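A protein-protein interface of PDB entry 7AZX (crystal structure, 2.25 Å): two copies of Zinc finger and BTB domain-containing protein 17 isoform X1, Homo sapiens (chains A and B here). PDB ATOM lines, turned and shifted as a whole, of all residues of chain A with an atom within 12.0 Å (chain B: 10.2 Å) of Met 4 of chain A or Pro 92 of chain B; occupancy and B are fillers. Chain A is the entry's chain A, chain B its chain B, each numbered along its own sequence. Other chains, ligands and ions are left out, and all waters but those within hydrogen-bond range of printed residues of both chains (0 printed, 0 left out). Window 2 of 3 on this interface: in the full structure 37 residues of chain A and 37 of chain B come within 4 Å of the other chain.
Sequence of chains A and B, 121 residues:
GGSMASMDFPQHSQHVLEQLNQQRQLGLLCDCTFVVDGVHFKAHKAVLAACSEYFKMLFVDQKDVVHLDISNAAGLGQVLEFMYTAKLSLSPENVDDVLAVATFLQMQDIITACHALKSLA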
ATOM      1  N   SER A   3      -6.603   7.516 -13.344  1.00  0.00           N
ATOM      2  CA  SER A   3      -6.588   8.706 -14.185  1.00  0.00           C
ATOM      3  C   SER A   3      -7.979   9.317 -14.322  1.00  0.00           C
ATOM      4  O   SER A   3      -8.556   9.797 -13.344  1.00  0.00           O
ATOM      5  CB  SER A   3      -6.023   8.379 -15.571  1.00  0.00           C
ATOM      6  OG  SER A   3      -4.608   8.438 -15.574  1.00  0.00           O
ATOM      7  N   MET A   4      -8.510   9.296 -15.541  1.00  0.00           N
ATOM      8  CA  MET A   4      -9.780   9.933 -15.864  1.00  0.00           C
ATOM      9  C   MET A   4     -10.839   8.871 -16.124  1.00  0.00           C
ATOM     10  O   MET A   4     -10.598   7.917 -16.873  1.00  0.00           O
ATOM     11  CB  MET A   4      -9.633  10.845 -17.085  1.00  0.00           C
ATOM     12  CG  MET A   4     -10.819  11.769 -17.322  1.00  0.00           C
ATOM     13  SD  MET A   4     -10.535  12.948 -18.658  1.00  0.00           S
ATOM     14  CE  MET A   4     -11.672  14.255 -18.203  1.00  0.00           C
ATOM     15  N   ALA A   5     -12.008   9.041 -15.508  1.00  0.00           N
ATOM     16  CA  ALA A   5     -13.120   8.115 -15.681  1.00  0.00           C
ATOM     17  C   ALA A   5     -14.388   8.748 -15.130  1.00  0.00           C
ATOM     18  O   ALA A   5     -14.342   9.522 -14.169  1.00  0.00           O
ATOM     19  CB  ALA A   5     -12.856   6.773 -14.984  1.00  0.00           C
ATOM     20  N   SER A   6     -15.515   8.408 -15.750  1.00  0.00           N
ATOM     21  CA  SER A   6     -16.836   8.817 -15.294  1.00  0.00           C
ATOM     22  C   SER A   6     -17.584   7.598 -14.775  1.00  0.00           C
ATOM     23  O   SER A   6     -17.503   6.514 -15.360  1.00  0.00           O
ATOM     24  CB  SER A   6     -17.632   9.480 -16.421  1.00  0.00           C
ATOM     25  OG  SER A   6     -17.195  10.809 -16.643  1.00  0.00           O
ATOM     26  N   MET A   7     -18.308   7.773 -13.675  1.00  0.00           N
ATOM     27  CA  MET A   7     -19.017   6.679 -13.027  1.00  0.00           C
ATOM     28  C   MET A   7     -20.456   7.077 -12.735  1.00  0.00           C
ATOM     29  O   MET A   7     -20.730   8.212 -12.330  1.00  0.00           O
ATOM     30  CB  MET A   7     -18.326   6.249 -11.724  1.00  0.00           C
ATOM     31  CG  MET A   7     -16.807   6.220 -11.795  1.00  0.00           C
ATOM     32  SD  MET A   7     -16.054   5.981 -10.178  1.00  0.00           S
ATOM     33  CE  MET A   7     -17.216   4.824  -9.459  1.00  0.00           C
ATOM     34  N   ASP A   8     -21.371   6.132 -12.941  1.00  0.00           N
ATOM     35  CA  ASP A   8     -22.801   6.338 -12.740  1.00  0.00           C
ATOM     36  C   ASP A   8     -23.322   5.312 -11.744  1.00  0.00           C
ATOM     37  O   ASP A   8     -23.032   4.117 -11.869  1.00  0.00           O
ATOM     38  CB  ASP A   8     -23.558   6.230 -14.070  1.00  0.00           C
ATOM     39  CG  ASP A   8     -25.064   6.352 -13.903  1.00  0.00           C
ATOM     40  OD1 ASP A   8     -25.572   7.491 -13.814  1.00  0.00           O
ATOM     41  OD2 ASP A   8     -25.743   5.305 -13.871  1.00  0.00           O
ATOM     42  N   GLN B  78     -17.969  18.774  -7.441  1.00  0.00           N
ATOM     43  CA  GLN B  78     -18.196  17.433  -7.971  1.00  0.00           C
ATOM     44  C   GLN B  78     -18.953  16.559  -6.980  1.00  0.00           C
ATOM     45  O   GLN B  78     -19.735  15.694  -7.391  1.00  0.00           O
ATOM     46  CB  GLN B  78     -16.865  16.780  -8.345  1.00  0.00           C
ATOM     47  CG  GLN B  78     -16.398  17.090  -9.759  1.00  0.00           C
ATOM     48  CD  GLN B  78     -17.304  16.490 -10.816  1.00  0.00           C
ATOM     49  OE1 GLN B  78     -17.927  15.450 -10.601  1.00  0.00           O
ATOM     50  NE2 GLN B  78     -17.384  17.148 -11.968  1.00  0.00           N
ATOM     51  N   LEU B  88     -20.567  10.729 -11.172  1.00  0.00           N
ATOM     52  CA  LEU B  88     -19.313  11.218 -10.613  1.00  0.00           C
ATOM     53  C   LEU B  88     -18.262  11.236 -11.713  1.00  0.00           C
ATOM     54  O   LEU B  88     -17.930  10.187 -12.277  1.00  0.00           O
ATOM     55  CB  LEU B  88     -18.857  10.343  -9.443  1.00  0.00           C
ATOM     56  CG  LEU B  88     -17.736  10.902  -8.566  1.00  0.00           C
ATOM     57  CD1 LEU B  88     -18.234  12.079  -7.741  1.00  0.00           C
ATOM     58  CD2 LEU B  88     -17.171   9.813  -7.666  1.00  0.00           C
ATOM     59  N   SER B  89     -17.744  12.423 -12.016  1.00  0.00           N
ATOM     60  CA  SER B  89     -16.715  12.607 -13.032  1.00  0.00           C
ATOM     61  C   SER B  89     -15.397  12.913 -12.336  1.00  0.00           C
ATOM     62  O   SER B  89     -15.291  13.911 -11.616  1.00  0.00           O
ATOM     63  CB  SER B  89     -17.091  13.730 -13.996  1.00  0.00           C
ATOM     64  OG  SER B  89     -18.430  13.594 -14.439  1.00  0.00           O
ATOM     65  N   LEU B  90     -14.399  12.059 -12.551  1.00  0.00           N
ATOM     66  CA  LEU B  90     -13.108  12.204 -11.897  1.00  0.00           C
ATOM     67  C   LEU B  90     -11.996  12.249 -12.932  1.00  0.00           C
ATOM     68  O   LEU B  90     -12.034  11.531 -13.936  1.00  0.00           O
ATOM     69  CB  LEU B  90     -12.856  11.064 -10.906  1.00  0.00           C
ATOM     70  CG  LEU B  90     -14.004  10.778  -9.937  1.00  0.00           C
ATOM     71  CD1 LEU B  90     -14.098   9.292  -9.629  1.00  0.00           C
ATOM     72  CD2 LEU B  90     -13.850  11.594  -8.661  1.00  0.00           C
ATOM     73  N   SER B  91     -11.005  13.097 -12.672  1.00  0.00           N
ATOM     74  CA  SER B  91      -9.841  13.270 -13.527  1.00  0.00           C
ATOM     75  C   SER B  91      -8.637  13.511 -12.631  1.00  0.00           C
ATOM     76  O   SER B  91      -8.804  13.947 -11.485  1.00  0.00           O
ATOM     77  CB  SER B  91     -10.035  14.436 -14.511  1.00  0.00           C
ATOM     78  OG  SER B  91     -10.063  15.684 -13.842  1.00  0.00           O
ATOM     79  N   PRO B  92      -7.410  13.238 -13.115  1.00  0.00           N
ATOM     80  CA  PRO B  92      -6.225  13.369 -12.252  1.00  0.00           C
ATOM     81  C   PRO B  92      -6.059  14.746 -11.627  1.00  0.00           C
ATOM     82  O   PRO B  92      -5.249  14.920 -10.712  1.00  0.00           O
ATOM     83  CB  PRO B  92      -5.064  13.054 -13.205  1.00  0.00           C
ATOM     84  CG  PRO B  92      -5.660  12.205 -14.254  1.00  0.00           C
ATOM     85  CD  PRO B  92      -7.067  12.689 -14.438  1.00  0.00           C
ATOM     86  N   GLU B  93      -6.821  15.729 -12.103  1.00  0.00           N
ATOM     87  CA  GLU B  93      -6.770  17.076 -11.554  1.00  0.00           C
ATOM     88  C   GLU B  93      -7.732  17.295 -10.391  1.00  0.00           C
ATOM     89  O   GLU B  93      -7.681  18.360  -9.768  1.00  0.00           O
ATOM     90  CB  GLU B  93      -7.064  18.110 -12.649  1.00  0.00           C
ATOM     91  CG  GLU B  93      -5.952  18.274 -13.675  1.00  0.00           C
ATOM     92  CD  GLU B  93      -5.924  17.150 -14.690  1.00  0.00           C
ATOM     93  OE1 GLU B  93      -6.928  16.415 -14.789  1.00  0.00           O
ATOM     94  OE2 GLU B  93      -4.896  16.999 -15.382  1.00  0.00           O
ATOM     95  N   ASN B  94      -8.604  16.331 -10.073  1.00  0.00           N
ATOM     96  CA  ASN B  94      -9.598  16.560  -9.033  1.00  0.00           C
ATOM     97  C   ASN B  94      -9.954  15.332  -8.200  1.00  0.00           C
ATOM     98  O   ASN B  94     -10.797  15.451  -7.303  1.00  0.00           O
ATOM     99  CB  ASN B  94     -10.887  17.140  -9.647  1.00  0.00           C
ATOM    100  CG  ASN B  94     -11.769  16.077 -10.270  1.00  0.00           C
ATOM    101  OD1 ASN B  94     -11.284  15.104 -10.849  1.00  0.00           O
ATOM    102  ND2 ASN B  94     -13.078  16.245 -10.130  1.00  0.00           N
ATOM    103  N   VAL B  95      -9.338  14.172  -8.446  1.00  0.00           N
ATOM    104  CA  VAL B  95      -9.667  12.968  -7.685  1.00  0.00           C
ATOM    105  C   VAL B  95      -9.219  13.116  -6.234  1.00  0.00           C
ATOM    106  O   VAL B  95      -9.871  12.614  -5.306  1.00  0.00           O
ATOM    107  CB  VAL B  95      -9.022  11.741  -8.359  1.00  0.00           C
ATOM    108  CG1 VAL B  95      -7.535  11.990  -8.557  1.00  0.00           C
ATOM    109  CG2 VAL B  95      -9.272  10.467  -7.550  1.00  0.00           C
ATOM    110  N   ASP B  96      -8.075  13.773  -6.020  1.00  0.00           N
ATOM    111  CA  ASP B  96      -7.610  14.065  -4.667  1.00  0.00           C
ATOM    112  C   ASP B  96      -8.480  15.112  -3.986  1.00  0.00           C
ATOM    113  O   ASP B  96      -8.707  15.034  -2.774  1.00  0.00           O
ATOM    114  CB  ASP B  96      -6.148  14.530  -4.689  1.00  0.00           C
ATOM    115  CG  ASP B  96      -5.216  13.501  -5.303  1.00  0.00           C
ATOM    116  OD1 ASP B  96      -5.465  12.288  -5.122  1.00  0.00           O
ATOM    117  OD2 ASP B  96      -4.209  13.892  -5.930  1.00  0.00           O
ATOM    118  N   ASP B  97      -8.973  16.095  -4.742  1.00  0.00           N
ATOM    119  CA  ASP B  97      -9.843  17.105  -4.151  1.00  0.00           C
ATOM    120  C   ASP B  97     -11.227  16.547  -3.846  1.00  0.00           C
ATOM    121  O   ASP B  97     -11.896  17.017  -2.918  1.00  0.00           O
ATOM    122  CB  ASP B  97      -9.949  18.319  -5.076  1.00  0.00           C
ATOM    123  CG  ASP B  97      -8.776  19.267  -4.934  1.00  0.00           C
ATOM    124  OD1 ASP B  97      -8.240  19.395  -3.813  1.00  0.00           O
ATOM    125  OD2 ASP B  97      -8.395  19.890  -5.947  1.00  0.00           O
ATOM    126  N   VAL B  98     -11.671  15.548  -4.609  1.00  0.00           N
ATOM    127  CA  VAL B  98     -12.976  14.946  -4.363  1.00  0.00           C
ATOM    128  C   VAL B  98     -12.919  14.002  -3.168  1.00  0.00           C
ATOM    129  O   VAL B  98     -13.823  13.996  -2.327  1.00  0.00           O
ATOM    130  CB  VAL B  98     -13.479  14.234  -5.633  1.00  0.00           C
ATOM    131  CG1 VAL B  98     -14.635  13.304  -5.304  1.00  0.00           C
ATOM    132  CG2 VAL B  98     -13.909  15.252  -6.679  1.00  0.00           C
ATOM    133  N   ALA B 113     -14.741   5.040  -4.694  1.00  0.00           N
ATOM    134  CA  ALA B 113     -14.629   5.336  -6.120  1.00  0.00           C
ATOM    135  C   ALA B 113     -13.274   5.950  -6.451  1.00  0.00           C
ATOM    136  O   ALA B 113     -12.617   5.553  -7.421  1.00  0.00           O
ATOM    137  CB  ALA B 113     -15.762   6.267  -6.545  1.00  0.00           C
ATOM    138  N   CYS B 114     -12.840   6.925  -5.651  1.00  0.00           N
ATOM    139  CA  CYS B 114     -11.552   7.573  -5.861  1.00  0.00           C
ATOM    140  C   CYS B 114     -10.388   6.798  -5.255  1.00  0.00           C
ATOM    141  O   CYS B 114      -9.241   7.010  -5.666  1.00  0.00           O
ATOM    142  CB  CYS B 114     -11.584   8.991  -5.287  1.00  0.00           C
ATOM    143  SG  CYS B 114     -13.172   9.844  -5.471  1.00  0.00           S
ATOM    144  N   ALA B 116      -9.713   3.788  -5.798  1.00  0.00           N
ATOM    145  CA  ALA B 116      -9.160   2.980  -6.880  1.00  0.00           C
ATOM    146  C   ALA B 116      -8.271   3.818  -7.791  1.00  0.00           C
ATOM    147  O   ALA B 116      -7.125   3.446  -8.072  1.00  0.00           O
ATOM    148  CB  ALA B 116     -10.292   2.331  -7.676  1.00  0.00           C
ATOM    149  N   LEU B 117      -8.781   4.951  -8.260  1.00  0.00           N
ATOM    150  CA  LEU B 117      -8.032   5.815  -9.164  1.00  0.00           C
ATOM    151  C   LEU B 117      -7.106   6.748  -8.389  1.00  0.00           C
ATOM    152  O   LEU B 117      -6.096   6.315  -7.835  1.00  0.00           O
ATOM    153  CB  LEU B 117      -8.983   6.630 -10.046  1.00  0.00           C
ATOM    154  CG  LEU B 117      -9.737   5.884 -11.152  1.00  0.00           C
ATOM    155  CD1 LEU B 117     -10.955   5.145 -10.608  1.00  0.00           C
ATOM    156  CD2 LEU B 117     -10.140   6.844 -12.263  1.00  0.00           C
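The backbone NH (N) of Ala 5 of chain A sits at hydrogen-bond distance from the backbone carbonyl oxygen (O) of Leu 90 of chain B, 2.9 Å away. The backbone carbonyl oxygen of Met 7 of chain A sits at hydrogen-bond distance from the backbone NH of Leu 88 of chain B (2.8 Å).
The side-chain amide oxygen (OE1) of Gln 78 of chain B sits close to the backbone carbonyl oxygen (O) of Ser 89 of chain B (3.2 Å). The side-chain carboxylate of Glu 93 of chain B sits at hydrogen-bond distance from the side-chain hydroxyl of Ser 91 of chain B, 3.4 Å away. The backbone NH of Ser 91 of chain B sits at hydrogen-bond distance from the side-chain amide oxygen of Asn 94 of chain B (2.7 Å).
O of Ser 3 of chain A touches CA of Ser 91 of chain B, 3.7 Å away. Ser 3 of chain A touches Pro 92 of chain B. Leu 117 of chain B touches Ser 3 of chain A (CD2 to O, 3.5 Å). O of Leu 90 of chain B touches CA of Met 4 of chain A, 3.4 Å away. N of Met 4 of chain A touches CD of Pro 92 of chain B, 3.8 Å away. Ser 89 of chain B touches Ala 5 of chain A (C to O, 3.996 Å). CB of Ala 5 of chain A touches CD2 of Leu 117 of chain B, 3.8 Å away. OG of Ser 6 of chain A touches OG of Ser 89 of chain B, at 3.8 Å. SD of Met 7 of chain A touches CD1 of Leu 90 of chain B, at 3.9 Å. Met 7 of chain A touches Ala 113 of chain B.
Of chain B, only Leu 90 (3.9 Å), Ser 91 (3.7 Å), Pro 92 (3.4 Å) and Leu 117 (3.5 Å) come within 4 Å of Ser 3 of chain A. Met 4 of chain A touches just these residues of chain B: Leu 90 (3.4 Å), Ser 91 (3.95 Å) and Pro 92 (3.8 Å). Of the printed residues of chain B, Ala 5 of chain A touches Ser 89, Leu 90 and Leu 117. Of the printed residues of chain A, Leu 88 of chain B touches Ser 6 (3.5 Å) and Met 7 (2.8 Å). Of the printed residues of chain A, Ser 89 of chain B touches Ala 5 and Ser 6. Of the printed residues of chain A, Ser 91 of chain B touches Ser 3 (3.7 Å) and Met 4 (3.95 Å). Of chain A, only Ser 3 and Met 4 come within 4 Å of Pro 92 of chain B. No residue of chain A comes within 4 Å of Glu 93 of chain B. No residue of chain A comes within 4 Å of Asn 94 of chain B. Val 95 of chain B touches none of the printed residues of chain A. Val 98 of chain B touches none of the printed residues of chain A. Of the printed residues of chain A, Ala 113 of chain B touches Met 7 (3.6 Å). Cys 114 of chain B touches none of the printed residues of chain A. Printed residues of chain A within 4 Å of Leu 117 of chain B: Ser 3 and Ala 5. The nearest residue of chain A that does not touch Pro 92 of chain B is Ala 5 of chain A (6.2 Å). The nearest printed residue of chain A that does not touch Ala 113 of chain B is Ala 5 of chain A (7.7 Å).
Of the 6 printed residues of chain A, 5 touch a printed residue of chain B. Printed residues of chain A that touch a printed residue of chain B: Ser 3, Met 4, Ala 5, Ser 6 and Met 7. Hydrophobic or aromatic side chains of chain A that line the printed part of chain B: Met 4, Ala 5 and Met 7. Hydrophobic or aromatic side chains of chain B within 4 Å of the printed part of chain A: Leu 90, Pro 92, Ala 113 and Leu 117. Among the printed residues, no Asp or Glu carboxylate lies within 4 Å of a Lys or Arg side-chain nitrogen of the other chain.
No position is printed for both chains. Of the 15 pairs that touch across the chains among the printed residues, none has its exchanged pair printed and touching as well.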
